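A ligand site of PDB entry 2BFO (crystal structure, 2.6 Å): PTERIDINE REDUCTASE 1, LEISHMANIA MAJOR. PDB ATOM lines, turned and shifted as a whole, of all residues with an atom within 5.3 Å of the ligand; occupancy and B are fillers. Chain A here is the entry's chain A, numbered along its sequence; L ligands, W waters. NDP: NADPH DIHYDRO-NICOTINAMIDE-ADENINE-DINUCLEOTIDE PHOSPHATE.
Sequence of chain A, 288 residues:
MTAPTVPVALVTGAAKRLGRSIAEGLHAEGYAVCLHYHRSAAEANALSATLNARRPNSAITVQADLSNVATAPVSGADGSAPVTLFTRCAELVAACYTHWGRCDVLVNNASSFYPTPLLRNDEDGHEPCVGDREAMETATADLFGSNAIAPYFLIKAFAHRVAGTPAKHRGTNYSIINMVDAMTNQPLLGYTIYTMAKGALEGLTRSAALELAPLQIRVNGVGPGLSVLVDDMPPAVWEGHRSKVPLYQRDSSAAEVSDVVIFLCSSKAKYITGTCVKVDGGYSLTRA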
ATOM      1  N   GLY A  13      10.063  14.787 -29.374  1.00  0.00           N
ATOM      2  CA  GLY A  13       9.135  15.723 -29.996  1.00  0.00           C
ATOM      3  C   GLY A  13       9.187  15.654 -31.508  1.00  0.00           C
ATOM      4  O   GLY A  13       9.211  16.668 -32.207  1.00  0.00           O
ATOM      5  N   ALA A  15       6.906  14.418 -33.630  1.00  0.00           N
ATOM      6  CA  ALA A  15       5.605  14.407 -34.286  1.00  0.00           C
ATOM      7  C   ALA A  15       5.374  15.493 -35.350  1.00  0.00           C
ATOM      8  O   ALA A  15       4.795  15.217 -36.401  1.00  0.00           O
ATOM      9  CB  ALA A  15       4.496  14.439 -33.258  1.00  0.00           C
ATOM     10  N   LYS A  16       5.826  16.716 -35.101  1.00  0.00           N
ATOM     11  CA  LYS A  16       5.601  17.767 -36.085  1.00  0.00           C
ATOM     12  C   LYS A  16       6.667  18.835 -36.194  1.00  0.00           C
ATOM     13  O   LYS A  16       7.682  18.793 -35.532  1.00  0.00           O
ATOM     14  CB  LYS A  16       4.234  18.417 -35.849  1.00  0.00           C
ATOM     15  CG  LYS A  16       3.893  18.748 -34.394  1.00  0.00           C
ATOM     16  CD  LYS A  16       2.390  18.553 -34.155  1.00  0.00           C
ATOM     17  CE  LYS A  16       1.838  19.496 -33.065  1.00  0.00           C
ATOM     18  NZ  LYS A  16       0.474  19.006 -32.702  1.00  0.00           N
ATOM     19  N   ARG A  17       6.422  19.793 -37.078  1.00  0.00           N
ATOM     20  CA  ARG A  17       7.271  20.979 -37.176  1.00  0.00           C
ATOM     21  C   ARG A  17       8.769  20.625 -37.331  1.00  0.00           C
ATOM     22  O   ARG A  17       9.092  19.775 -38.168  1.00  0.00           O
ATOM     23  CB  ARG A  17       6.994  21.915 -35.985  1.00  0.00           C
ATOM     24  CG  ARG A  17       5.606  22.559 -36.072  1.00  0.00           C
ATOM     25  CD  ARG A  17       5.165  23.255 -34.809  1.00  0.00           C
ATOM     26  NE  ARG A  17       6.132  24.290 -34.448  1.00  0.00           N
ATOM     27  CZ  ARG A  17       6.180  25.504 -35.008  1.00  0.00           C
ATOM     28  NH1 ARG A  17       5.300  25.856 -35.935  1.00  0.00           N
ATOM     29  NH2 ARG A  17       7.125  26.350 -34.635  1.00  0.00           N
ATOM     30  N   LEU A  18       9.661  21.262 -36.548  1.00  0.00           N
ATOM     31  CA  LEU A  18      11.104  21.004 -36.623  1.00  0.00           C
ATOM     32  C   LEU A  18      11.488  19.577 -36.291  1.00  0.00           C
ATOM     33  O   LEU A  18      12.361  19.013 -36.949  1.00  0.00           O
ATOM     34  CB  LEU A  18      11.947  21.948 -35.735  1.00  0.00           C
ATOM     35  CG  LEU A  18      11.915  23.488 -35.876  1.00  0.00           C
ATOM     36  CD1 LEU A  18      13.178  24.142 -35.335  1.00  0.00           C
ATOM     37  CD2 LEU A  18      11.616  23.992 -37.283  1.00  0.00           C
ATOM     38  N   GLY A  19      10.854  18.992 -35.276  1.00  0.00           N
ATOM     39  CA  GLY A  19      11.131  17.615 -34.929  1.00  0.00           C
ATOM     40  C   GLY A  19      10.833  16.618 -36.053  1.00  0.00           C
ATOM     41  O   GLY A  19      11.614  15.716 -36.305  1.00  0.00           O
ATOM     42  N   HIS A  36       9.841  10.078 -30.794  1.00  0.00           N
ATOM     43  CA  HIS A  36       9.181  10.266 -29.485  1.00  0.00           C
ATOM     44  C   HIS A  36       8.091  11.316 -29.607  1.00  0.00           C
ATOM     45  O   HIS A  36       8.180  12.252 -30.409  1.00  0.00           O
ATOM     46  CB  HIS A  36      10.179  10.670 -28.367  1.00  0.00           C
ATOM     47  CG  HIS A  36       9.554  11.427 -27.230  1.00  0.00           C
ATOM     48  ND1 HIS A  36       9.211  12.763 -27.306  1.00  0.00           N
ATOM     49  CD2 HIS A  36       9.150  11.019 -25.996  1.00  0.00           C
ATOM     50  CE1 HIS A  36       8.633  13.144 -26.183  1.00  0.00           C
ATOM     51  NE2 HIS A  36       8.586  12.115 -25.368  1.00  0.00           N
ATOM     52  N   TYR A  37       7.060  11.170 -28.796  1.00  0.00           N
ATOM     53  CA  TYR A  37       5.971  12.139 -28.747  1.00  0.00           C
ATOM     54  C   TYR A  37       5.351  12.165 -27.353  1.00  0.00           C
ATOM     55  O   TYR A  37       5.466  11.194 -26.587  1.00  0.00           O
ATOM     56  CB  TYR A  37       4.914  11.811 -29.792  1.00  0.00           C
ATOM     57  CG  TYR A  37       4.097  10.599 -29.424  1.00  0.00           C
ATOM     58  CD1 TYR A  37       4.563   9.297 -29.686  1.00  0.00           C
ATOM     59  CD2 TYR A  37       2.862  10.744 -28.793  1.00  0.00           C
ATOM     60  CE1 TYR A  37       3.828   8.205 -29.344  1.00  0.00           C
ATOM     61  CE2 TYR A  37       2.130   9.628 -28.453  1.00  0.00           C
ATOM     62  CZ  TYR A  37       2.618   8.372 -28.754  1.00  0.00           C
ATOM     63  OH  TYR A  37       1.930   7.246 -28.427  1.00  0.00           O
ATOM     64  N   HIS A  38       4.706  13.277 -27.023  1.00  0.00           N
ATOM     65  CA  HIS A  38       4.028  13.382 -25.757  1.00  0.00           C
ATOM     66  C   HIS A  38       2.526  13.298 -26.023  1.00  0.00           C
ATOM     67  O   HIS A  38       1.904  12.320 -25.646  1.00  0.00           O
ATOM     68  CB  HIS A  38       4.425  14.669 -25.041  1.00  0.00           C
ATOM     69  CG  HIS A  38       3.792  14.823 -23.699  1.00  0.00           C
ATOM     70  ND1 HIS A  38       3.443  16.048 -23.172  1.00  0.00           N
ATOM     71  CD2 HIS A  38       3.390  13.896 -22.796  1.00  0.00           C
ATOM     72  CE1 HIS A  38       2.890  15.869 -21.995  1.00  0.00           C
ATOM     73  NE2 HIS A  38       2.839  14.572 -21.739  1.00  0.00           N
ATOM     74  N   ARG A  39       1.964  14.317 -26.692  1.00  0.00           N
ATOM     75  CA  ARG A  39       0.525  14.390 -26.937  1.00  0.00           C
ATOM     76  C   ARG A  39       0.098  14.185 -28.400  1.00  0.00           C
ATOM     77  O   ARG A  39      -1.065  13.927 -28.681  1.00  0.00           O
ATOM     78  CB  ARG A  39      -0.038  15.717 -26.411  1.00  0.00           C
ATOM     79  CG  ARG A  39       0.004  15.831 -24.859  1.00  0.00           C
ATOM     80  CD  ARG A  39      -0.121  17.240 -24.320  1.00  0.00           C
ATOM     81  NE  ARG A  39       0.043  17.285 -22.873  1.00  0.00           N
ATOM     82  CZ  ARG A  39       0.453  18.376 -22.182  1.00  0.00           C
ATOM     83  NH1 ARG A  39       0.733  19.506 -22.826  1.00  0.00           N
ATOM     84  NH2 ARG A  39       0.591  18.335 -20.858  1.00  0.00           N
ATOM     85  N   SER A  40       1.032  14.289 -29.336  1.00  0.00           N
ATOM     86  CA  SER A  40       0.701  14.173 -30.735  1.00  0.00           C
ATOM     87  C   SER A  40       0.795  12.738 -31.245  1.00  0.00           C
ATOM     88  O   SER A  40       1.543  12.445 -32.191  1.00  0.00           O
ATOM     89  CB  SER A  40       1.593  15.084 -31.556  1.00  0.00           C
ATOM     90  OG  SER A  40       1.387  16.431 -31.196  1.00  0.00           O
ATOM     91  N   ALA A  64       6.062   9.746 -24.142  1.00  0.00           N
ATOM     92  CA  ALA A  64       6.656  10.102 -22.864  1.00  0.00           C
ATOM     93  C   ALA A  64       6.526  11.563 -22.507  1.00  0.00           C
ATOM     94  O   ALA A  64       6.845  12.437 -23.324  1.00  0.00           O
ATOM     95  CB  ALA A  64       8.103   9.687 -22.816  1.00  0.00           C
ATOM     96  N   ASP A  65       6.069  11.817 -21.283  1.00  0.00           N
ATOM     97  CA  ASP A  65       6.069  13.152 -20.727  1.00  0.00           C
ATOM     98  C   ASP A  65       7.473  13.361 -20.212  1.00  0.00           C
ATOM     99  O   ASP A  65       7.914  12.623 -19.366  1.00  0.00           O
ATOM    100  CB  ASP A  65       5.084  13.238 -19.568  1.00  0.00           C
ATOM    101  CG  ASP A  65       5.058  14.621 -18.929  1.00  0.00           C
ATOM    102  OD1 ASP A  65       5.751  15.535 -19.408  1.00  0.00           O
ATOM    103  OD2 ASP A  65       4.352  14.874 -17.957  1.00  0.00           O
ATOM    104  N   LEU A  66       8.151  14.382 -20.715  1.00  0.00           N
ATOM    105  CA  LEU A  66       9.506  14.666 -20.288  1.00  0.00           C
ATOM    106  C   LEU A  66       9.541  15.747 -19.216  1.00  0.00           C
ATOM    107  O   LEU A  66      10.603  16.187 -18.793  1.00  0.00           O
ATOM    108  CB  LEU A  66      10.382  15.036 -21.480  1.00  0.00           C
ATOM    109  CG  LEU A  66      10.477  13.949 -22.555  1.00  0.00           C
ATOM    110  CD1 LEU A  66      11.368  14.306 -23.777  1.00  0.00           C
ATOM    111  CD2 LEU A  66      10.922  12.643 -21.944  1.00  0.00           C
ATOM    112  N   SER A  67       8.376  16.173 -18.757  1.00  0.00           N
ATOM    113  CA  SER A  67       8.339  17.115 -17.665  1.00  0.00           C
ATOM    114  C   SER A  67       9.010  16.474 -16.465  1.00  0.00           C
ATOM    115  O   SER A  67       8.937  15.272 -16.285  1.00  0.00           O
ATOM    116  CB  SER A  67       6.917  17.511 -17.355  1.00  0.00           C
ATOM    117  OG  SER A  67       6.889  18.163 -16.117  1.00  0.00           O
ATOM    118  N   ASN A 108      17.720  16.136 -28.879  1.00  0.00           N
ATOM    119  CA  ASN A 108      16.876  16.718 -27.846  1.00  0.00           C
ATOM    120  C   ASN A 108      16.167  17.923 -28.435  1.00  0.00           C
ATOM    121  O   ASN A 108      16.685  19.048 -28.376  1.00  0.00           O
ATOM    122  CB  ASN A 108      17.698  17.113 -26.630  1.00  0.00           C
ATOM    123  CG  ASN A 108      18.207  15.892 -25.856  1.00  0.00           C
ATOM    124  OD1 ASN A 108      17.417  15.048 -25.418  1.00  0.00           O
ATOM    125  ND2 ASN A 108      19.527  15.778 -25.708  1.00  0.00           N
ATOM    126  N   ASN A 109      14.999  17.644 -29.035  1.00  0.00           N
ATOM    127  CA  ASN A 109      14.176  18.632 -29.739  1.00  0.00           C
ATOM    128  C   ASN A 109      12.932  19.060 -28.983  1.00  0.00           C
ATOM    129  O   ASN A 109      12.509  20.193 -29.104  1.00  0.00           O
ATOM    130  CB  ASN A 109      13.816  18.116 -31.134  1.00  0.00           C
ATOM    131  CG  ASN A 109      12.883  19.011 -31.884  1.00  0.00           C
ATOM    132  OD1 ASN A 109      13.283  20.022 -32.421  1.00  0.00           O
ATOM    133  ND2 ASN A 109      11.629  18.632 -31.942  1.00  0.00           N
ATOM    134  N   ALA A 110      12.346  18.141 -28.218  1.00  0.00           N
ATOM    135  CA  ALA A 110      11.105  18.401 -27.456  1.00  0.00           C
ATOM    136  C   ALA A 110      11.287  19.618 -26.586  1.00  0.00           C
ATOM    137  O   ALA A 110      12.338  19.769 -25.987  1.00  0.00           O
ATOM    138  CB  ALA A 110      10.705  17.207 -26.585  1.00  0.00           C
ATOM    139  N   SER A 111      10.259  20.472 -26.526  1.00  0.00           N
ATOM    140  CA  SER A 111      10.384  21.715 -25.780  1.00  0.00           C
ATOM    141  C   SER A 111       9.043  22.391 -25.509  1.00  0.00           C
ATOM    142  O   SER A 111       8.263  22.688 -26.429  1.00  0.00           O
ATOM    143  CB  SER A 111      11.308  22.665 -26.548  1.00  0.00           C
ATOM    144  OG  SER A 111      11.079  24.021 -26.187  1.00  0.00           O
ATOM    145  N   SER A 112       8.785  22.656 -24.250  1.00  0.00           N
ATOM    146  CA  SER A 112       7.605  23.418 -23.882  1.00  0.00           C
ATOM    147  C   SER A 112       7.955  24.909 -23.897  1.00  0.00           C
ATOM    148  O   SER A 112       9.081  25.287 -23.547  1.00  0.00           O
ATOM    149  CB  SER A 112       7.014  22.938 -22.535  1.00  0.00           C
ATOM    150  OG  SER A 112       7.904  23.141 -21.438  1.00  0.00           O
ATOM    151  N   ASP A 142       7.711  21.353 -16.069  1.00  0.00           N
ATOM    152  CA  ASP A 142       7.491  21.155 -17.491  1.00  0.00           C
ATOM    153  C   ASP A 142       8.548  21.864 -18.335  1.00  0.00           C
ATOM    154  O   ASP A 142       9.210  21.244 -19.168  1.00  0.00           O
ATOM    155  CB  ASP A 142       6.077  21.587 -17.868  1.00  0.00           C
ATOM    156  CG  ASP A 142       5.745  21.267 -19.297  1.00  0.00           C
ATOM    157  OD1 ASP A 142       5.906  20.083 -19.679  1.00  0.00           O
ATOM    158  OD2 ASP A 142       5.343  22.141 -20.099  1.00  0.00           O
ATOM    159  N   SER A 146      11.489  19.365 -20.000  1.00  0.00           N
ATOM    160  CA  SER A 146      11.541  19.211 -21.435  1.00  0.00           C
ATOM    161  C   SER A 146      12.781  19.833 -22.039  1.00  0.00           C
ATOM    162  O   SER A 146      13.428  19.219 -22.865  1.00  0.00           O
ATOM    163  CB  SER A 146      10.246  19.761 -22.077  1.00  0.00           C
ATOM    164  OG  SER A 146      10.142  21.157 -21.944  1.00  0.00           O
ATOM    165  N   ASN A 147      13.132  21.038 -21.619  1.00  0.00           N
ATOM    166  CA  ASN A 147      14.173  21.793 -22.247  1.00  0.00           C
ATOM    167  C   ASN A 147      15.568  21.525 -21.707  1.00  0.00           C
ATOM    168  O   ASN A 147      16.561  21.859 -22.389  1.00  0.00           O
ATOM    169  CB  ASN A 147      13.880  23.310 -22.104  1.00  0.00           C
ATOM    170  CG  ASN A 147      12.763  23.773 -23.014  1.00  0.00           C
ATOM    171  OD1 ASN A 147      12.909  23.743 -24.233  1.00  0.00           O
ATOM    172  ND2 ASN A 147      11.655  24.173 -22.430  1.00  0.00           N
ATOM    173  N   MET A 179      18.582  21.158 -29.304  1.00  0.00           N
ATOM    174  CA  MET A 179      17.960  22.299 -29.928  1.00  0.00           C
ATOM    175  C   MET A 179      17.910  23.462 -28.943  1.00  0.00           C
ATOM    176  O   MET A 179      17.152  23.431 -27.974  1.00  0.00           O
ATOM    177  CB  MET A 179      16.569  21.948 -30.437  1.00  0.00           C
ATOM    178  CG  MET A 179      16.554  20.842 -31.441  1.00  0.00           C
ATOM    179  SD  MET A 179      17.643  21.178 -32.865  1.00  0.00           S
ATOM    180  CE  MET A 179      16.620  22.479 -33.778  1.00  0.00           C
ATOM    181  N   VAL A 180      18.754  24.462 -29.163  1.00  0.00           N
ATOM    182  CA  VAL A 180      18.790  25.647 -28.308  1.00  0.00           C
ATOM    183  C   VAL A 180      18.021  26.824 -28.920  1.00  0.00           C
ATOM    184  O   VAL A 180      17.101  26.626 -29.715  1.00  0.00           O
ATOM    185  CB  VAL A 180      20.240  26.023 -27.886  1.00  0.00           C
ATOM    186  CG1 VAL A 180      20.826  24.921 -27.023  1.00  0.00           C
ATOM    187  CG2 VAL A 180      21.154  26.272 -29.112  1.00  0.00           C
ATOM    188  N   ASP A 181      18.362  28.043 -28.551  1.00  0.00           N
ATOM    189  CA  ASP A 181      17.625  29.204 -29.055  1.00  0.00           C
ATOM    190  C   ASP A 181      18.622  30.274 -29.341  1.00  0.00           C
ATOM    191  O   ASP A 181      19.307  30.740 -28.420  1.00  0.00           O
ATOM    192  CB  ASP A 181      16.636  29.699 -28.015  1.00  0.00           C
ATOM    193  CG  ASP A 181      15.696  30.782 -28.550  1.00  0.00           C
ATOM    194  OD1 ASP A 181      16.128  31.678 -29.294  1.00  0.00           O
ATOM    195  OD2 ASP A 181      14.493  30.847 -28.253  1.00  0.00           O
ATOM    196  N   ALA A 182      18.725  30.689 -30.601  1.00  0.00           N
ATOM    197  CA  ALA A 182      19.690  31.721 -30.974  1.00  0.00           C
ATOM    198  C   ALA A 182      19.387  33.100 -30.309  1.00  0.00           C
ATOM    199  O   ALA A 182      20.255  33.977 -30.252  1.00  0.00           O
ATOM    200  CB  ALA A 182      19.763  31.850 -32.509  1.00  0.00           C
ATOM    201  N   TYR A 194      11.690  29.652 -19.440  1.00  0.00           N
ATOM    202  CA  TYR A 194      12.040  29.046 -20.685  1.00  0.00           C
ATOM    203  C   TYR A 194      13.456  29.424 -21.060  1.00  0.00           C
ATOM    204  O   TYR A 194      14.299  28.568 -21.427  1.00  0.00           O
ATOM    205  CB  TYR A 194      11.098  29.496 -21.798  1.00  0.00           C
ATOM    206  CG  TYR A 194      11.699  29.311 -23.186  1.00  0.00           C
ATOM    207  CD1 TYR A 194      11.648  28.066 -23.835  1.00  0.00           C
ATOM    208  CD2 TYR A 194      12.345  30.370 -23.860  1.00  0.00           C
ATOM    209  CE1 TYR A 194      12.187  27.887 -25.077  1.00  0.00           C
ATOM    210  CE2 TYR A 194      12.876  30.195 -25.125  1.00  0.00           C
ATOM    211  CZ  TYR A 194      12.806  28.941 -25.716  1.00  0.00           C
ATOM    212  OH  TYR A 194      13.342  28.733 -26.970  1.00  0.00           O
ATOM    213  N   LYS A 198      16.782  27.039 -21.496  1.00  0.00           N
ATOM    214  CA  LYS A 198      17.661  27.049 -22.648  1.00  0.00           C
ATOM    215  C   LYS A 198      19.133  27.349 -22.304  1.00  0.00           C
ATOM    216  O   LYS A 198      20.057  26.786 -22.906  1.00  0.00           O
ATOM    217  CB  LYS A 198      17.146  28.012 -23.714  1.00  0.00           C
ATOM    218  CG  LYS A 198      15.929  27.505 -24.471  1.00  0.00           C
ATOM    219  CD  LYS A 198      16.163  26.162 -25.127  1.00  0.00           C
ATOM    220  CE  LYS A 198      14.921  25.819 -25.952  1.00  0.00           C
ATOM    221  NZ  LYS A 198      14.946  24.457 -26.487  1.00  0.00           N
ATOM    222  N   PRO A 224      17.698  27.862 -33.468  1.00  0.00           N
ATOM    223  CA  PRO A 224      16.904  28.600 -34.436  1.00  0.00           C
ATOM    224  C   PRO A 224      16.637  29.999 -33.922  1.00  0.00           C
ATOM    225  O   PRO A 224      16.841  30.262 -32.751  1.00  0.00           O
ATOM    226  CB  PRO A 224      15.612  27.772 -34.543  1.00  0.00           C
ATOM    227  CG  PRO A 224      16.002  26.438 -34.053  1.00  0.00           C
ATOM    228  CD  PRO A 224      16.953  26.723 -32.921  1.00  0.00           C
ATOM    229  N   GLY A 225      16.218  30.874 -34.827  1.00  0.00           N
ATOM    230  CA  GLY A 225      15.770  32.205 -34.501  1.00  0.00           C
ATOM    231  C   GLY A 225      14.254  32.205 -34.549  1.00  0.00           C
ATOM    232  O   GLY A 225      13.581  31.986 -33.520  1.00  0.00           O
ATOM    233  N   LEU A 226      13.716  32.464 -35.744  1.00  0.00           N
ATOM    234  CA  LEU A 226      12.287  32.320 -36.002  1.00  0.00           C
ATOM    235  C   LEU A 226      12.093  31.258 -37.074  1.00  0.00           C
ATOM    236  O   LEU A 226      12.541  31.432 -38.197  1.00  0.00           O
ATOM    237  CB  LEU A 226      11.665  33.640 -36.446  1.00  0.00           C
ATOM    238  CG  LEU A 226      11.798  34.821 -35.471  1.00  0.00           C
ATOM    239  CD1 LEU A 226      11.110  36.072 -36.083  1.00  0.00           C
ATOM    240  CD2 LEU A 226      11.306  34.505 -34.041  1.00  0.00           C
ATOM    241  N   SER A 227      11.454  30.141 -36.702  1.00  0.00           N
ATOM    242  CA  SER A 227      11.150  29.066 -37.645  1.00  0.00           C
ATOM    243  C   SER A 227       9.693  28.675 -37.604  1.00  0.00           C
ATOM    244  O   SER A 227       9.146  28.434 -36.528  1.00  0.00           O
ATOM    245  CB  SER A 227      11.990  27.839 -37.400  1.00  0.00           C
ATOM    246  OG  SER A 227      13.327  28.131 -37.678  1.00  0.00           O
ATOM    247  N   VAL A 228       9.089  28.595 -38.798  1.00  0.00           N
ATOM    248  CA  VAL A 228       7.688  28.223 -38.955  1.00  0.00           C
ATOM    249  C   VAL A 228       6.872  28.914 -37.878  1.00  0.00           C
ATOM    250  O   VAL A 228       6.136  28.299 -37.086  1.00  0.00           O
ATOM    251  CB  VAL A 228       7.530  26.687 -38.964  1.00  0.00           C
ATOM    252  CG1 VAL A 228       6.092  26.289 -39.324  1.00  0.00           C
ATOM    253  CG2 VAL A 228       8.439  26.110 -39.994  1.00  0.00           C
HETATM  254  PA  NDP L   1       7.519  22.855 -30.840  1.00  0.00           P
HETATM  255  O1A NDP L   1       7.198  24.071 -30.066  1.00  0.00           O
HETATM  256  O2A NDP L   1       6.533  22.569 -31.943  1.00  0.00           O
HETATM  257  O5B NDP L   1       7.614  21.612 -29.841  1.00  0.00           O
HETATM  258  C5B NDP L   1       8.198  20.412 -30.248  1.00  0.00           C
HETATM  259  C4B NDP L   1       7.700  19.250 -29.401  1.00  0.00           C
HETATM  260  O4B NDP L   1       8.123  19.261 -28.049  1.00  0.00           O
HETATM  261  C3B NDP L   1       6.176  19.274 -29.333  1.00  0.00           C
HETATM  262  O3B NDP L   1       5.691  18.720 -30.535  1.00  0.00           O
HETATM  263  C2B NDP L   1       5.883  18.440 -28.088  1.00  0.00           C
HETATM  264  O2B NDP L   1       5.474  17.103 -28.413  1.00  0.00           O
HETATM  265  C1B NDP L   1       7.211  18.422 -27.342  1.00  0.00           C
HETATM  266  N9A NDP L   1       7.074  18.717 -25.905  1.00  0.00           N
HETATM  267  C8A NDP L   1       6.756  19.890 -25.306  1.00  0.00           C
HETATM  268  N7A NDP L   1       6.712  19.724 -23.981  1.00  0.00           N
HETATM  269  C5A NDP L   1       6.994  18.446 -23.728  1.00  0.00           C
HETATM  270  C6A NDP L   1       7.082  17.735 -22.548  1.00  0.00           C
HETATM  271  N6A NDP L   1       6.774  18.281 -21.381  1.00  0.00           N
HETATM  272  N1A NDP L   1       7.374  16.392 -22.587  1.00  0.00           N
HETATM  273  C2A NDP L   1       7.585  15.764 -23.794  1.00  0.00           C
HETATM  274  N3A NDP L   1       7.493  16.461 -24.957  1.00  0.00           N
HETATM  275  C4A NDP L   1       7.209  17.794 -24.919  1.00  0.00           C
HETATM  276  O3  NDP L   1       9.042  23.010 -31.336  1.00  0.00           O
HETATM  277  PN  NDP L   1       9.565  23.671 -32.698  1.00  0.00           P
HETATM  278  O1N NDP L   1       8.983  25.006 -32.876  1.00  0.00           O
HETATM  279  O2N NDP L   1       9.385  22.656 -33.763  1.00  0.00           O
HETATM  280  O5D NDP L   1      11.128  23.790 -32.369  1.00  0.00           O
HETATM  281  C5D NDP L   1      11.906  22.654 -32.039  1.00  0.00           C
HETATM  282  C4D NDP L   1      13.089  23.027 -31.147  1.00  0.00           C
HETATM  283  O4D NDP L   1      13.676  24.235 -31.613  1.00  0.00           O
HETATM  284  C3D NDP L   1      12.666  23.277 -29.716  1.00  0.00           C
HETATM  285  O3D NDP L   1      13.644  22.787 -28.825  1.00  0.00           O
HETATM  286  C2D NDP L   1      12.600  24.795 -29.620  1.00  0.00           C
HETATM  287  O2D NDP L   1      12.849  25.220 -28.306  1.00  0.00           O
HETATM  288  C1D NDP L   1      13.686  25.228 -30.595  1.00  0.00           C
HETATM  289  N1N NDP L   1      13.435  26.585 -31.158  1.00  0.00           N
HETATM  290  C2N NDP L   1      12.434  26.780 -32.082  1.00  0.00           C
HETATM  291  C3N NDP L   1      12.204  28.043 -32.620  1.00  0.00           C
HETATM  292  C7N NDP L   1      11.132  28.269 -33.644  1.00  0.00           C
HETATM  293  O7N NDP L   1      10.966  29.544 -34.120  1.00  0.00           O
HETATM  294  N7N NDP L   1      10.392  27.235 -34.052  1.00  0.00           N
HETATM  295  C4N NDP L   1      12.982  29.116 -32.206  1.00  0.00           C
HETATM  296  C5N NDP L   1      14.043  28.910 -31.192  1.00  0.00           C
HETATM  297  C6N NDP L   1      14.217  27.632 -30.711  1.00  0.00           C
HETATM  298  P2B NDP L   1       3.965  16.552 -28.486  1.00  0.00           P
HETATM  299  O1X NDP L   1       4.030  15.133 -28.891  1.00  0.00           O
HETATM  300  O2X NDP L   1       3.340  16.656 -27.112  1.00  0.00           O
HETATM  301  O3X NDP L   1       3.253  17.456 -29.509  1.00  0.00           O
HETATM  302  O   HOH W   1      15.218  21.065 -26.557  1.00  0.00           O
HETATM  303  O   HOH W   2       6.165  15.386 -30.713  1.00  0.00           O
HETATM  304  O   HOH W   3       6.156  23.314 -27.727  1.00  0.00           O
HETATM  305  O   HOH W   4       6.824  17.748 -32.874  1.00  0.00           O
HETATM  306  O   HOH W   5       9.173  20.217 -33.386  1.00  0.00           O
HETATM  307  O   HOH W   6       9.867  31.805 -32.441  1.00  0.00           O
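A nitrogen (N6A) of the ligand lies within hydrogen-bond range of the side-chain carboxylate of Asp 142 (2.6 Å). An oxygen (O7N) of the ligand lies within hydrogen-bond range of the backbone NH (N) of Ser 227. The backbone carbonyl oxygen of Ser 227 sits at hydrogen-bond distance from a nitrogen (N7N) of the ligand (3.0 Å). N of Ser 40 sits at hydrogen-bond distance from O1X of the ligand, 3.1 Å away. The side-chain hydroxyl of Ser 40 sits at hydrogen-bond distance from an oxygen (O3X) of the ligand (2.7 Å). The backbone NH (N) of His 38 lies within hydrogen-bond range of an oxygen (O1X) of the ligand (2.7 Å). The backbone NH (N) of Arg 39 lies within hydrogen-bond range of an oxygen (O2X) of the ligand (2.7 Å). O of Asn 109 lies within hydrogen-bond range of O3D of the ligand, at 2.8 Å. N1A of the ligand lies within hydrogen-bond range of N of Leu 66. The side-chain amino group of Lys 198 sits at hydrogen-bond distance from an oxygen (O2D) of the ligand, at 2.9 Å. The backbone NH of Ser 111 is in hydrogen-bond range of an oxygen (O4B) of the ligand (2.9 Å). The side-chain hydroxyl of Ser 111 lies within hydrogen-bond range of an oxygen (O2D) of the ligand, at 3.0 Å. An oxygen (O1N) of the ligand lies within salt-bridge range of the guanidinium group (NH2) of Arg 17 (2.9 Å). The backbone NH (N) of Leu 18 is in hydrogen-bond range of an oxygen (O2N) of the ligand (3.1 Å).
The side-chain carboxylate of Asp 142 sits at hydrogen-bond distance from the side-chain hydroxyl of Ser 112 (3.1 Å). The backbone carbonyl oxygen (O) of Gly 13 sits at hydrogen-bond distance from the side-chain amide nitrogen (ND2) of Asn 109 (3.1 Å). ND2 of Asn 109 lies close to N of Gly 19. O of Val 228 lies within hydrogen-bond range of NH1 of Arg 17 (2.8 Å). NE2 of His 36 sits at hydrogen-bond distance from O of Ala 64, at 2.7 Å. N of Met 179 lies within hydrogen-bond range of O of Asn 108 (3.0 Å). O of Pro 224 sits at hydrogen-bond distance from N of Ala 182 (2.9 Å). The side-chain hydroxyl of Tyr 194 sits at hydrogen-bond distance from the side-chain carboxylate of Asp 181.
CA of Gly 13 touches C4B of the ligand (3.9 Å). His 36 touches the ligand. Tyr 37 touches the ligand (CB to O1X, 3.6 Å). Ala 64 touches the ligand. Asp 65 touches the ligand. Ser 67 touches the ligand (N to N6A, 3.7 Å). CA of Ala 110 touches O4B of the ligand, at 3.2 Å. Ser 112 touches the ligand (CB to N7A, 3.5 Å). CB of Ser 146 touches C6A of the ligand, 3.8 Å away. Met 179 touches the ligand (CB to O3D, 3.4 Å). Val 180 touches the ligand (O to C6N, 3.2 Å). OD2 of Asp 181 touches C5N of the ligand, 3.5 Å away. Tyr 194 touches the ligand. Pro 224 touches the ligand (O to C5N, 3.5 Å). O of Gly 225 touches C4N of the ligand (3.2 Å). Leu 226 touches the ligand (C to O7N, 3.6 Å). Hydrophobic or aromatic side chains within 4 Å of the ligand: Leu 18, His 36, Tyr 37, His 38, Leu 66, Ala 110, Met 179 and Pro 224. Of the 34 residues printed, 27 come within 4 Å of the ligand.
Water W3 lies within hydrogen-bond range of the backbone carbonyl oxygen of Ser 111 (2.6 Å) and an oxygen (O1A) of the ligand (2.7 Å). Water W4 lies within hydrogen-bond range of the backbone NH (N) of Lys 16 (2.6 Å), the backbone carbonyl oxygen (O) of Gly 13 (2.7 Å), an oxygen (O3B) of the ligand (2.8 Å) and the backbone NH (N) of Ala 15 (3.4 Å). Water W2 lies within hydrogen-bond range of an oxygen (O1X) of the ligand (2.8 Å) and the backbone NH (N) of Ala 15 (3.2 Å).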
